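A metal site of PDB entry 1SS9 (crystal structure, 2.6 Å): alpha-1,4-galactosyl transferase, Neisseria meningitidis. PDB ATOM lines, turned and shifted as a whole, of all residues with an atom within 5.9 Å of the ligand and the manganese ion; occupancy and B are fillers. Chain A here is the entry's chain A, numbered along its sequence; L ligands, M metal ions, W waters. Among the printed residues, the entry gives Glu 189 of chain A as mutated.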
ATOM      1  N   ALA A   6      23.432  21.446  29.106  1.00  0.00           N
ATOM      2  CA  ALA A   6      22.337  21.644  28.164  1.00  0.00           C
ATOM      3  C   ALA A   6      21.223  20.703  28.588  1.00  0.00           C
ATOM      4  O   ALA A   6      21.473  19.524  28.821  1.00  0.00           O
ATOM      5  CB  ALA A   6      22.782  21.311  26.756  1.00  0.00           C
ATOM      6  N   ALA A   7      20.003  21.224  28.716  1.00  0.00           N
ATOM      7  CA  ALA A   7      18.888  20.371  29.099  1.00  0.00           C
ATOM      8  C   ALA A   7      17.516  20.941  28.802  1.00  0.00           C
ATOM      9  O   ALA A   7      17.354  22.148  28.549  1.00  0.00           O
ATOM     10  CB  ALA A   7      18.984  20.060  30.591  1.00  0.00           C
ATOM     11  N   ASP A   8      16.518  20.058  28.802  1.00  0.00           N
ATOM     12  CA  ASP A   8      15.148  20.457  28.615  1.00  0.00           C
ATOM     13  C   ASP A   8      14.408  20.135  29.916  1.00  0.00           C
ATOM     14  O   ASP A   8      14.994  19.569  30.849  1.00  0.00           O
ATOM     15  CB  ASP A   8      14.484  19.767  27.421  1.00  0.00           C
ATOM     16  CG  ASP A   8      14.828  18.301  27.307  1.00  0.00           C
ATOM     17  OD1 ASP A   8      15.126  17.671  28.346  1.00  0.00           O
ATOM     18  OD2 ASP A   8      14.776  17.788  26.168  1.00  0.00           O
ATOM     19  N   ASN A  10      12.535  17.838  31.033  1.00  0.00           N
ATOM     20  CA  ASN A  10      12.649  16.452  31.496  1.00  0.00           C
ATOM     21  C   ASN A  10      13.878  16.160  32.357  1.00  0.00           C
ATOM     22  O   ASN A  10      13.800  15.380  33.315  1.00  0.00           O
ATOM     23  CB  ASN A  10      12.642  15.527  30.264  1.00  0.00           C
ATOM     24  CG  ASN A  10      12.407  14.067  30.626  1.00  0.00           C
ATOM     25  OD1 ASN A  10      11.527  13.735  31.423  1.00  0.00           O
ATOM     26  ND2 ASN A  10      13.190  13.181  30.012  1.00  0.00           N
ATOM     27  N   TYR A  11      14.999  16.780  32.027  1.00  0.00           N
ATOM     28  CA  TYR A  11      16.249  16.559  32.746  1.00  0.00           C
ATOM     29  C   TYR A  11      16.576  17.627  33.795  1.00  0.00           C
ATOM     30  O   TYR A  11      17.675  17.632  34.340  1.00  0.00           O
ATOM     31  CB  TYR A  11      17.413  16.448  31.757  1.00  0.00           C
ATOM     32  CG  TYR A  11      17.721  15.036  31.300  1.00  0.00           C
ATOM     33  CD1 TYR A  11      16.728  14.057  31.247  1.00  0.00           C
ATOM     34  CD2 TYR A  11      19.021  14.679  30.954  1.00  0.00           C
ATOM     35  CE1 TYR A  11      17.034  12.756  30.844  1.00  0.00           C
ATOM     36  CE2 TYR A  11      19.336  13.390  30.564  1.00  0.00           C
ATOM     37  CZ  TYR A  11      18.346  12.439  30.512  1.00  0.00           C
ATOM     38  OH  TYR A  11      18.667  11.172  30.111  1.00  0.00           O
ATOM     39  N   ILE A  76      19.046   7.516  18.582  1.00  0.00           N
ATOM     40  CA  ILE A  76      19.215   7.007  19.936  1.00  0.00           C
ATOM     41  C   ILE A  76      18.062   7.501  20.818  1.00  0.00           C
ATOM     42  O   ILE A  76      17.985   8.675  21.179  1.00  0.00           O
ATOM     43  CB  ILE A  76      20.577   7.461  20.511  1.00  0.00           C
ATOM     44  CG1 ILE A  76      21.696   6.973  19.585  1.00  0.00           C
ATOM     45  CG2 ILE A  76      20.775   6.889  21.906  1.00  0.00           C
ATOM     46  CD1 ILE A  76      23.066   7.505  19.922  1.00  0.00           C
ATOM     47  N   HIS A  78      16.991   7.313  24.123  1.00  0.00           N
ATOM     48  CA  HIS A  78      17.115   8.032  25.389  1.00  0.00           C
ATOM     49  C   HIS A  78      17.667   9.450  25.288  1.00  0.00           C
ATOM     50  O   HIS A  78      17.795  10.134  26.302  1.00  0.00           O
ATOM     51  CB  HIS A  78      17.928   7.224  26.400  1.00  0.00           C
ATOM     52  CG  HIS A  78      19.403   7.235  26.141  1.00  0.00           C
ATOM     53  ND1 HIS A  78      19.983   6.612  25.054  1.00  0.00           N
ATOM     54  CD2 HIS A  78      20.424   7.792  26.842  1.00  0.00           C
ATOM     55  CE1 HIS A  78      21.288   6.799  25.087  1.00  0.00           C
ATOM     56  NE2 HIS A  78      21.578   7.506  26.159  1.00  0.00           N
ATOM     57  N   ILE A  79      17.974   9.888  24.076  1.00  0.00           N
ATOM     58  CA  ILE A  79      18.494  11.237  23.874  1.00  0.00           C
ATOM     59  C   ILE A  79      17.495  12.103  23.141  1.00  0.00           C
ATOM     60  O   ILE A  79      16.886  11.657  22.163  1.00  0.00           O
ATOM     61  CB  ILE A  79      19.805  11.184  23.084  1.00  0.00           C
ATOM     62  CG1 ILE A  79      20.883  10.488  23.924  1.00  0.00           C
ATOM     63  CG2 ILE A  79      20.243  12.589  22.692  1.00  0.00           C
ATOM     64  CD1 ILE A  79      22.010   9.900  23.112  1.00  0.00           C
ATOM     65  N   SER A  80      17.313  13.339  23.592  1.00  0.00           N
ATOM     66  CA  SER A  80      16.376  14.258  22.935  1.00  0.00           C
ATOM     67  C   SER A  80      17.098  15.280  22.070  1.00  0.00           C
ATOM     68  O   SER A  80      18.323  15.404  22.102  1.00  0.00           O
ATOM     69  CB  SER A  80      15.517  14.983  23.982  1.00  0.00           C
ATOM     70  OG  SER A  80      16.319  15.804  24.809  1.00  0.00           O
ATOM     71  N   THR A  82      17.636  18.162  22.376  1.00  0.00           N
ATOM     72  CA  THR A  82      18.488  19.076  23.114  1.00  0.00           C
ATOM     73  C   THR A  82      19.977  18.734  23.010  1.00  0.00           C
ATOM     74  O   THR A  82      20.851  19.571  23.244  1.00  0.00           O
ATOM     75  CB  THR A  82      18.070  19.145  24.591  1.00  0.00           C
ATOM     76  OG1 THR A  82      16.755  19.721  24.674  1.00  0.00           O
ATOM     77  CG2 THR A  82      19.027  20.003  25.384  1.00  0.00           C
ATOM     78  N   THR A  83      20.273  17.490  22.624  1.00  0.00           N
ATOM     79  CA  THR A  83      21.653  17.046  22.500  1.00  0.00           C
ATOM     80  C   THR A  83      22.473  17.829  21.435  1.00  0.00           C
ATOM     81  O   THR A  83      23.703  17.858  21.495  1.00  0.00           O
ATOM     82  CB  THR A  83      21.702  15.523  22.175  1.00  0.00           C
ATOM     83  OG1 THR A  83      23.020  15.020  22.415  1.00  0.00           O
ATOM     84  CG2 THR A  83      21.309  15.272  20.697  1.00  0.00           C
ATOM     85  N   ARG A  86      24.622  22.127  21.891  1.00  0.00           N
ATOM     86  CA  ARG A  86      26.019  22.442  22.113  1.00  0.00           C
ATOM     87  C   ARG A  86      26.688  22.935  20.809  1.00  0.00           C
ATOM     88  O   ARG A  86      27.711  23.627  20.853  1.00  0.00           O
ATOM     89  CB  ARG A  86      26.742  21.203  22.664  1.00  0.00           C
ATOM     90  CG  ARG A  86      26.810  20.018  21.706  1.00  0.00           C
ATOM     91  CD  ARG A  86      27.230  18.734  22.424  1.00  0.00           C
ATOM     92  NE  ARG A  86      26.086  17.982  22.943  1.00  0.00           N
ATOM     93  CZ  ARG A  86      26.183  16.879  23.675  1.00  0.00           C
ATOM     94  NH1 ARG A  86      27.382  16.398  23.973  1.00  0.00           N
ATOM     95  NH2 ARG A  86      25.092  16.264  24.091  1.00  0.00           N
ATOM     96  N   TYR A 101      32.073  22.087  28.776  1.00  0.00           N
ATOM     97  CA  TYR A 101      30.774  21.470  28.552  1.00  0.00           C
ATOM     98  C   TYR A 101      30.667  20.079  29.204  1.00  0.00           C
ATOM     99  O   TYR A 101      31.535  19.220  29.021  1.00  0.00           O
ATOM    100  CB  TYR A 101      30.469  21.333  27.050  1.00  0.00           C
ATOM    101  CG  TYR A 101      29.156  20.627  26.780  1.00  0.00           C
ATOM    102  CD1 TYR A 101      27.948  21.337  26.700  1.00  0.00           C
ATOM    103  CD2 TYR A 101      29.102  19.236  26.688  1.00  0.00           C
ATOM    104  CE1 TYR A 101      26.719  20.687  26.552  1.00  0.00           C
ATOM    105  CE2 TYR A 101      27.872  18.571  26.538  1.00  0.00           C
ATOM    106  CZ  TYR A 101      26.692  19.306  26.476  1.00  0.00           C
ATOM    107  OH  TYR A 101      25.488  18.636  26.378  1.00  0.00           O
ATOM    108  N   LEU A 102      29.566  19.872  29.937  1.00  0.00           N
ATOM    109  CA  LEU A 102      29.303  18.603  30.609  1.00  0.00           C
ATOM    110  C   LEU A 102      27.921  18.045  30.260  1.00  0.00           C
ATOM    111  O   LEU A 102      26.948  18.802  30.184  1.00  0.00           O
ATOM    112  CB  LEU A 102      29.391  18.789  32.124  1.00  0.00           C
ATOM    113  CG  LEU A 102      30.764  19.115  32.673  1.00  0.00           C
ATOM    114  CD1 LEU A 102      30.761  19.110  34.213  1.00  0.00           C
ATOM    115  CD2 LEU A 102      31.738  18.083  32.133  1.00  0.00           C
ATOM    116  N   ASP A 103      27.853  16.733  30.046  1.00  0.00           N
ATOM    117  CA  ASP A 103      26.578  16.097  29.756  1.00  0.00           C
ATOM    118  C   ASP A 103      25.807  16.033  31.082  1.00  0.00           C
ATOM    119  O   ASP A 103      26.415  16.004  32.137  1.00  0.00           O
ATOM    120  CB  ASP A 103      26.792  14.686  29.211  1.00  0.00           C
ATOM    121  CG  ASP A 103      26.725  14.639  27.699  1.00  0.00           C
ATOM    122  OD1 ASP A 103      26.791  13.520  27.157  1.00  0.00           O
ATOM    123  OD2 ASP A 103      26.597  15.711  27.059  1.00  0.00           O
ATOM    124  N   ILE A 104      24.485  16.019  31.033  1.00  0.00           N
ATOM    125  CA  ILE A 104      23.711  15.961  32.272  1.00  0.00           C
ATOM    126  C   ILE A 104      24.000  14.692  33.066  1.00  0.00           C
ATOM    127  O   ILE A 104      24.060  14.729  34.294  1.00  0.00           O
ATOM    128  CB  ILE A 104      22.192  16.016  32.016  1.00  0.00           C
ATOM    129  CG1 ILE A 104      21.819  17.373  31.418  1.00  0.00           C
ATOM    130  CG2 ILE A 104      21.431  15.846  33.311  1.00  0.00           C
ATOM    131  CD1 ILE A 104      22.176  18.542  32.287  1.00  0.00           C
ATOM    132  N   ASP A 105      24.181  13.572  32.362  1.00  0.00           N
ATOM    133  CA  ASP A 105      24.432  12.281  33.011  1.00  0.00           C
ATOM    134  C   ASP A 105      25.853  12.055  33.544  1.00  0.00           C
ATOM    135  O   ASP A 105      26.337  10.918  33.521  1.00  0.00           O
ATOM    136  CB  ASP A 105      24.073  11.131  32.074  1.00  0.00           C
ATOM    137  CG  ASP A 105      24.936  11.095  30.824  1.00  0.00           C
ATOM    138  OD1 ASP A 105      25.722  12.047  30.629  1.00  0.00           O
ATOM    139  OD2 ASP A 105      24.838  10.144  30.028  1.00  0.00           O
ATOM    140  N   VAL A 106      26.517  13.120  33.999  1.00  0.00           N
ATOM    141  CA  VAL A 106      27.867  12.964  34.533  1.00  0.00           C
ATOM    142  C   VAL A 106      27.837  13.156  36.042  1.00  0.00           C
ATOM    143  O   VAL A 106      26.892  13.714  36.601  1.00  0.00           O
ATOM    144  CB  VAL A 106      28.882  13.982  33.945  1.00  0.00           C
ATOM    145  CG1 VAL A 106      28.886  13.899  32.445  1.00  0.00           C
ATOM    146  CG2 VAL A 106      28.566  15.393  34.425  1.00  0.00           C
ATOM    147  N   ASP A 130      36.845   8.071  23.179  1.00  0.00           N
ATOM    148  CA  ASP A 130      35.729   7.165  23.403  1.00  0.00           C
ATOM    149  C   ASP A 130      36.181   5.780  22.965  1.00  0.00           C
ATOM    150  O   ASP A 130      36.417   5.554  21.787  1.00  0.00           O
ATOM    151  CB  ASP A 130      34.523   7.595  22.579  1.00  0.00           C
ATOM    152  CG  ASP A 130      33.267   6.917  23.016  1.00  0.00           C
ATOM    153  OD1 ASP A 130      33.251   5.669  23.076  1.00  0.00           O
ATOM    154  OD2 ASP A 130      32.295   7.630  23.302  1.00  0.00           O
ATOM    155  N   ASN A 153      34.484  11.354  22.871  1.00  0.00           N
ATOM    156  CA  ASN A 153      33.133  11.385  23.400  1.00  0.00           C
ATOM    157  C   ASN A 153      32.767  12.867  23.632  1.00  0.00           C
ATOM    158  O   ASN A 153      33.592  13.645  24.084  1.00  0.00           O
ATOM    159  CB  ASN A 153      33.104  10.594  24.697  1.00  0.00           C
ATOM    160  CG  ASN A 153      31.740  10.535  25.313  1.00  0.00           C
ATOM    161  OD1 ASN A 153      31.342  11.416  26.079  1.00  0.00           O
ATOM    162  ND2 ASN A 153      30.985   9.486  24.967  1.00  0.00           N
ATOM    163  N   ALA A 154      31.529  13.245  23.340  1.00  0.00           N
ATOM    164  CA  ALA A 154      31.110  14.636  23.510  1.00  0.00           C
ATOM    165  C   ALA A 154      30.451  14.944  24.856  1.00  0.00           C
ATOM    166  O   ALA A 154      29.826  16.001  25.012  1.00  0.00           O
ATOM    167  CB  ALA A 154      30.169  15.039  22.361  1.00  0.00           C
ATOM    168  N   GLY A 155      30.599  14.042  25.820  1.00  0.00           N
ATOM    169  CA  GLY A 155      30.010  14.246  27.133  1.00  0.00           C
ATOM    170  C   GLY A 155      30.764  15.209  28.035  1.00  0.00           C
ATOM    171  O   GLY A 155      30.194  15.755  28.976  1.00  0.00           O
ATOM    172  N   VAL A 156      32.053  15.389  27.755  1.00  0.00           N
ATOM    173  CA  VAL A 156      32.890  16.288  28.539  1.00  0.00           C
ATOM    174  C   VAL A 156      33.717  17.074  27.532  1.00  0.00           C
ATOM    175  O   VAL A 156      34.413  16.494  26.704  1.00  0.00           O
ATOM    176  CB  VAL A 156      33.796  15.495  29.506  1.00  0.00           C
ATOM    177  CG1 VAL A 156      34.806  16.419  30.169  1.00  0.00           C
ATOM    178  CG2 VAL A 156      32.941  14.807  30.585  1.00  0.00           C
ATOM    179  N   TYR A 186      26.021   8.397  15.779  1.00  0.00           N
ATOM    180  CA  TYR A 186      26.137   8.963  17.110  1.00  0.00           C
ATOM    181  C   TYR A 186      25.764  10.440  17.203  1.00  0.00           C
ATOM    182  O   TYR A 186      26.095  11.122  18.167  1.00  0.00           O
ATOM    183  CB  TYR A 186      27.538   8.695  17.652  1.00  0.00           C
ATOM    184  CG  TYR A 186      27.891   7.230  17.630  1.00  0.00           C
ATOM    185  CD1 TYR A 186      28.767   6.712  16.671  1.00  0.00           C
ATOM    186  CD2 TYR A 186      27.350   6.341  18.571  1.00  0.00           C
ATOM    187  CE1 TYR A 186      29.091   5.363  16.653  1.00  0.00           C
ATOM    188  CE2 TYR A 186      27.666   4.993  18.559  1.00  0.00           C
ATOM    189  CZ  TYR A 186      28.540   4.497  17.596  1.00  0.00           C
ATOM    190  OH  TYR A 186      28.900   3.171  17.607  1.00  0.00           O
ATOM    191  N   GLN A 187      25.080  10.930  16.182  1.00  0.00           N
ATOM    192  CA  GLN A 187      24.587  12.290  16.179  1.00  0.00           C
ATOM    193  C   GLN A 187      25.600  13.403  16.444  1.00  0.00           C
ATOM    194  O   GLN A 187      26.702  13.406  15.887  1.00  0.00           O
ATOM    195  CB  GLN A 187      23.428  12.321  17.181  1.00  0.00           C
ATOM    196  CG  GLN A 187      22.452  11.179  16.867  1.00  0.00           C
ATOM    197  CD  GLN A 187      21.389  10.912  17.913  1.00  0.00           C
ATOM    198  OE1 GLN A 187      20.479  10.122  17.678  1.00  0.00           O
ATOM    199  NE2 GLN A 187      21.492  11.554  19.076  1.00  0.00           N
ATOM    200  N   ASP A 188      25.234  14.369  17.278  1.00  0.00           N
ATOM    201  CA  ASP A 188      26.110  15.494  17.577  1.00  0.00           C
ATOM    202  C   ASP A 188      27.549  15.068  17.870  1.00  0.00           C
ATOM    203  O   ASP A 188      28.482  15.848  17.680  1.00  0.00           O
ATOM    204  CB  ASP A 188      25.562  16.270  18.777  1.00  0.00           C
ATOM    205  CG  ASP A 188      25.619  15.458  20.040  1.00  0.00           C
ATOM    206  OD1 ASP A 188      24.821  14.498  20.154  1.00  0.00           O
ATOM    207  OD2 ASP A 188      26.463  15.760  20.905  1.00  0.00           O
ATOM    208  N   GLU A 189      27.710  13.833  18.335  1.00  0.00           N
ATOM    209  CA  GLU A 189      29.028  13.296  18.642  1.00  0.00           C
ATOM    210  C   GLU A 189      29.814  13.087  17.338  1.00  0.00           C
ATOM    211  O   GLU A 189      31.039  13.244  17.302  1.00  0.00           O
ATOM    212  CB  GLU A 189      28.881  11.980  19.416  1.00  0.00           C
ATOM    213  CG  GLU A 189      30.190  11.311  19.802  1.00  0.00           C
ATOM    214  CD  GLU A 189      30.021  10.309  20.934  1.00  0.00           C
ATOM    215  OE1 GLU A 189      29.799  10.743  22.085  1.00  0.00           O
ATOM    216  OE2 GLU A 189      30.115   9.084  20.679  1.00  0.00           O
ATOM    217  N   MET A 210      33.795   6.350  31.544  1.00  0.00           N
ATOM    218  CA  MET A 210      32.553   5.705  31.101  1.00  0.00           C
ATOM    219  C   MET A 210      32.548   4.181  31.340  1.00  0.00           C
ATOM    220  O   MET A 210      33.552   3.604  31.768  1.00  0.00           O
ATOM    221  CB  MET A 210      32.309   6.017  29.615  1.00  0.00           C
ATOM    222  CG  MET A 210      32.160   7.519  29.295  1.00  0.00           C
ATOM    223  SD  MET A 210      32.267   7.956  27.519  1.00  0.00           S
ATOM    224  CE  MET A 210      34.004   8.248  27.349  1.00  0.00           C
ATOM    225  N   HIS A 244      30.969   9.284  33.653  1.00  0.00           N
ATOM    226  CA  HIS A 244      29.999   9.598  32.604  1.00  0.00           C
ATOM    227  C   HIS A 244      29.167   8.361  32.318  1.00  0.00           C
ATOM    228  O   HIS A 244      29.639   7.405  31.700  1.00  0.00           O
ATOM    229  CB  HIS A 244      30.690  10.079  31.327  1.00  0.00           C
ATOM    230  CG  HIS A 244      29.728  10.528  30.263  1.00  0.00           C
ATOM    231  ND1 HIS A 244      30.079  10.628  28.934  1.00  0.00           N
ATOM    232  CD2 HIS A 244      28.421  10.897  30.338  1.00  0.00           C
ATOM    233  CE1 HIS A 244      29.033  11.033  28.236  1.00  0.00           C
ATOM    234  NE2 HIS A 244      28.010  11.205  29.062  1.00  0.00           N
ATOM    235  N   TYR A 245      27.909   8.389  32.738  1.00  0.00           N
ATOM    236  CA  TYR A 245      27.014   7.258  32.560  1.00  0.00           C
ATOM    237  C   TYR A 245      26.429   7.142  31.170  1.00  0.00           C
ATOM    238  O   TYR A 245      25.221   7.027  30.964  1.00  0.00           O
ATOM    239  CB  TYR A 245      25.937   7.298  33.634  1.00  0.00           C
ATOM    240  CG  TYR A 245      26.587   7.133  34.979  1.00  0.00           C
ATOM    241  CD1 TYR A 245      27.134   5.901  35.353  1.00  0.00           C
ATOM    242  CD2 TYR A 245      26.763   8.222  35.834  1.00  0.00           C
ATOM    243  CE1 TYR A 245      27.864   5.759  36.540  1.00  0.00           C
ATOM    244  CE2 TYR A 245      27.495   8.094  37.022  1.00  0.00           C
ATOM    245  CZ  TYR A 245      28.032   6.850  37.366  1.00  0.00           C
ATOM    246  OH  TYR A 245      28.778   6.724  38.507  1.00  0.00           O
ATOM    247  N   CYS A 246      27.362   7.166  30.217  1.00  0.00           N
ATOM    248  CA  CYS A 246      27.099   7.040  28.800  1.00  0.00           C
ATOM    249  C   CYS A 246      26.127   5.857  28.559  1.00  0.00           C
ATOM    250  O   CYS A 246      26.130   4.876  29.309  1.00  0.00           O
ATOM    251  CB  CYS A 246      28.443   6.800  28.113  1.00  0.00           C
ATOM    252  SG  CYS A 246      28.396   6.617  26.359  1.00  0.00           S
ATOM    253  N   GLY A 247      25.290   5.964  27.530  1.00  0.00           N
ATOM    254  CA  GLY A 247      24.349   4.896  27.225  1.00  0.00           C
ATOM    255  C   GLY A 247      22.972   4.971  27.880  1.00  0.00           C
ATOM    256  O   GLY A 247      22.664   5.910  28.611  1.00  0.00           O
ATOM    257  N   PRO A 248      22.116   3.975  27.646  1.00  0.00           N
ATOM    258  CA  PRO A 248      20.764   3.891  28.196  1.00  0.00           C
ATOM    259  C   PRO A 248      20.603   3.789  29.719  1.00  0.00           C
ATOM    260  O   PRO A 248      19.561   4.166  30.246  1.00  0.00           O
ATOM    261  CB  PRO A 248      20.186   2.662  27.488  1.00  0.00           C
ATOM    262  CG  PRO A 248      21.390   1.784  27.314  1.00  0.00           C
ATOM    263  CD  PRO A 248      22.403   2.789  26.806  1.00  0.00           C
ATOM    264  N   LYS A 250      21.203   5.008  33.332  1.00  0.00           N
ATOM    265  CA  LYS A 250      21.590   6.196  34.092  1.00  0.00           C
ATOM    266  C   LYS A 250      21.524   5.936  35.600  1.00  0.00           C
ATOM    267  O   LYS A 250      20.721   5.132  36.072  1.00  0.00           O
ATOM    268  CB  LYS A 250      20.670   7.359  33.717  1.00  0.00           C
ATOM    269  CG  LYS A 250      20.483   7.595  32.195  1.00  0.00           C
ATOM    270  CD  LYS A 250      21.780   8.022  31.503  1.00  0.00           C
ATOM    271  CE  LYS A 250      21.552   8.297  30.008  1.00  0.00           C
ATOM    272  NZ  LYS A 250      22.817   8.656  29.295  1.00  0.00           N
HETATM  273  N1  LIG L   1      18.970  15.425  27.022  1.00  0.00           N
HETATM  274  C1  LIG L   1      18.043  16.173  27.819  1.00  0.00           C
HETATM  275  N2  LIG L   1      16.837  15.464  28.094  1.00  0.00           N
HETATM  276  C2  LIG L   1      16.483  14.110  27.664  1.00  0.00           C
HETATM  277  C3  LIG L   1      17.473  13.378  26.866  1.00  0.00           C
HETATM  278  C4  LIG L   1      18.641  14.013  26.564  1.00  0.00           C
HETATM  279  O1  LIG L   1      18.267  17.279  28.197  1.00  0.00           O
HETATM  280  O2  LIG L   1      15.401  13.663  27.998  1.00  0.00           O
HETATM  281  C5  LIG L   1      20.381  15.912  26.538  1.00  0.00           C
HETATM  282  C6  LIG L   1      21.305  16.217  27.683  1.00  0.00           C
HETATM  283  O3  LIG L   1      22.028  17.373  27.395  1.00  0.00           O
HETATM  284  C7  LIG L   1      22.154  14.997  27.825  1.00  0.00           C
HETATM  285  C8  LIG L   1      22.531  14.866  26.381  1.00  0.00           C
HETATM  286  O4  LIG L   1      21.203  15.054  25.744  1.00  0.00           O
HETATM  287  O5  LIG L   1      23.360  15.200  28.558  1.00  0.00           O
HETATM  288  C9  LIG L   1      22.610  13.707  25.453  1.00  0.00           C
HETATM  289  O6  LIG L   1      22.499  12.321  25.920  1.00  0.00           O
HETATM  290  P1  LIG L   1      22.954  11.416  27.113  1.00  0.00           P
HETATM  291  O7  LIG L   1      23.751  12.066  28.172  1.00  0.00           O
HETATM  292  O8  LIG L   1      21.694  10.818  27.653  1.00  0.00           O
HETATM  293  O9  LIG L   1      23.782  10.723  25.959  1.00  0.00           O
HETATM  294  P2  LIG L   1      24.777   9.540  25.976  1.00  0.00           P
HETATM  295  O10 LIG L   1      25.830  10.032  26.868  1.00  0.00           O
HETATM  296  O11 LIG L   1      24.035   8.432  26.529  1.00  0.00           O
HETATM  297  O12 LIG L   1      25.515   9.058  24.661  1.00  0.00           O
HETATM  298  C10 LIG L   1      26.481   9.279  23.575  1.00  0.00           C
HETATM  299  C11 LIG L   1      27.598  10.203  24.082  1.00  0.00           C
HETATM  300  C12 LIG L   1      27.018  11.613  24.434  1.00  0.00           C
HETATM  301  C13 LIG L   1      26.388  12.284  23.163  1.00  0.00           C
HETATM  302  C14 LIG L   1      25.281  11.272  22.689  1.00  0.00           C
HETATM  303  C15 LIG L   1      24.641  11.795  21.414  1.00  0.00           C
HETATM  304  F1  LIG L   1      28.190   9.559  25.206  1.00  0.00           F
HETATM  305  O13 LIG L   1      28.057  12.468  24.911  1.00  0.00           O
HETATM  306  O14 LIG L   1      27.450  12.449  22.138  1.00  0.00           O
HETATM  307  O15 LIG L   1      25.840   9.926  22.372  1.00  0.00           O
HETATM  308  O16 LIG L   1      23.606  11.146  20.702  1.00  0.00           O
HETATM  309 MN    MN M   1      26.005  11.565  28.245  1.00  0.00          MN
HETATM  310  O   HOH W   1      24.533  18.917  29.281  1.00  0.00           O
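The side-chain hydroxyl (OG) of Ser 80 lies close to a nitrogen (N2) of the ligand, at 3.3 Å. The backbone NH (N) of Ile 104 is in hydrogen-bond range of an oxygen (O5) of the ligand. The side-chain amide nitrogen (NE2) of Gln 187 sits at hydrogen-bond distance from an oxygen (O16) of the ligand. A ring nitrogen (NE2) of His 78 sits at hydrogen-bond distance from an oxygen (O11) of the ligand. An oxygen (O3) of the ligand lies within hydrogen-bond range of the backbone carbonyl oxygen of Ala 6 (2.6 Å). The side-chain carboxylate (OE1) of Glu 189 is in hydrogen-bond range of an oxygen (O14) of the ligand, 2.9 Å away. N of Gly 155 sits at hydrogen-bond distance from O13 of the ligand (3.1 Å). NZ of Lys 250 lies within salt-bridge range of O8 of the ligand (2.9 Å). The backbone NH (N) of Gly 247 lies within hydrogen-bond range of an oxygen (O11) of the ligand (2.9 Å). A nitrogen (N2) of the ligand lies within hydrogen-bond range of the side-chain carboxylate (OD1) of Asp 8 (2.8 Å). O1 of the ligand sits at hydrogen-bond distance from N of Asp 8 (3.3 Å). The side-chain amide nitrogen (ND2) of Asn 10 is in hydrogen-bond range of an oxygen (O2) of the ligand (3.0 Å).
The side-chain carboxylate (OE1) of Glu 189 sits at hydrogen-bond distance from the backbone NH (N) of Ala 154, 3.3 Å away. The side-chain carboxylate (OE1) of Glu 189 sits at hydrogen-bond distance from the side-chain amide nitrogen (ND2) of Asn 153 (3.4 Å). N of Asp 103 lies within hydrogen-bond range of O of Gly 155 (2.8 Å). The side-chain hydroxyl (OH) of Tyr 101 sits close to the guanidinium group (NH2) of Arg 86. The side-chain amide oxygen (OE1) of Gln 187 sits at hydrogen-bond distance from the backbone NH (N) of Ile 76 (3.1 Å). The side-chain carboxylate (OD2) of Asp 103 lies within salt-bridge range of the guanidinium group (NH1) of Arg 86. A ring nitrogen (NE2) of His 78 sits at hydrogen-bond distance from the backbone carbonyl oxygen (O) of Gly 247 (3.1 Å). The side-chain sulfur of Met 210 lies within hydrogen-bond range of the side-chain amide nitrogen of Asn 153, at 3.2 Å.
F1 of the ligand lies close to ND2 of Asn 153, at 2.8 Å. A fluorine (F1) of the ligand lies close to the side-chain sulfur (SG) of Cys 246 (3.2 Å). Residues that only touch the ligand: Ala 7, Tyr 11, Ile 76, Ile 79, Thr 82, Thr 83, Arg 86, Tyr 101, Ala 154, Tyr 186 and Asp 188. Hydrophobic or aromatic side chains within 4 Å of the ligand: Ala 7, Tyr 11, Ile 76, His 78, Ile 79, Ile 104, Ala 154 and His 244. Within 4 Å of the ligand: Ala 6, Ala 7, Asp 8, Asn 10, Tyr 11, Ile 76, His 78, Ile 79, Ser 80, Thr 82, Thr 83, Arg 86, Tyr 101, Asp 103, Ile 104, Asp 105, Asn 153, Ala 154, Gly 155, Tyr 186, Gln 187, Asp 188, Glu 189, His 244, Cys 246, Gly 247 and Lys 250. The nearest printed residue that does not touch the ligand is Tyr 245 (4.8 Å).
Three residues have an atom within 4 Å of the manganese ion: Asp 103, Asp 105 and His 244. The nearest printed residue that does not touch the manganese ion is Lys 250 (4.4 Å).
The manganese ion is bound by an oxygen (O10) of the ligand, a ring nitrogen (NE2) of His 244, an oxygen (O7) of the ligand, the side-chain carboxylate (OD1) of Asp 103, the side-chain carboxylate (OD1) of Asp 105 and the side-chain carboxylate (OD2) of Asp 105. The manganese ion has six donor atoms within binding distance.
Water W1 lies within hydrogen-bond range of O of Leu 102 (2.6 Å), N of Ala 6 (2.8 Å), OH of Tyr 101 (3.1 Å), N of Ile 104 (3.4 Å) and O3 of the ligand (3.5 Å).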
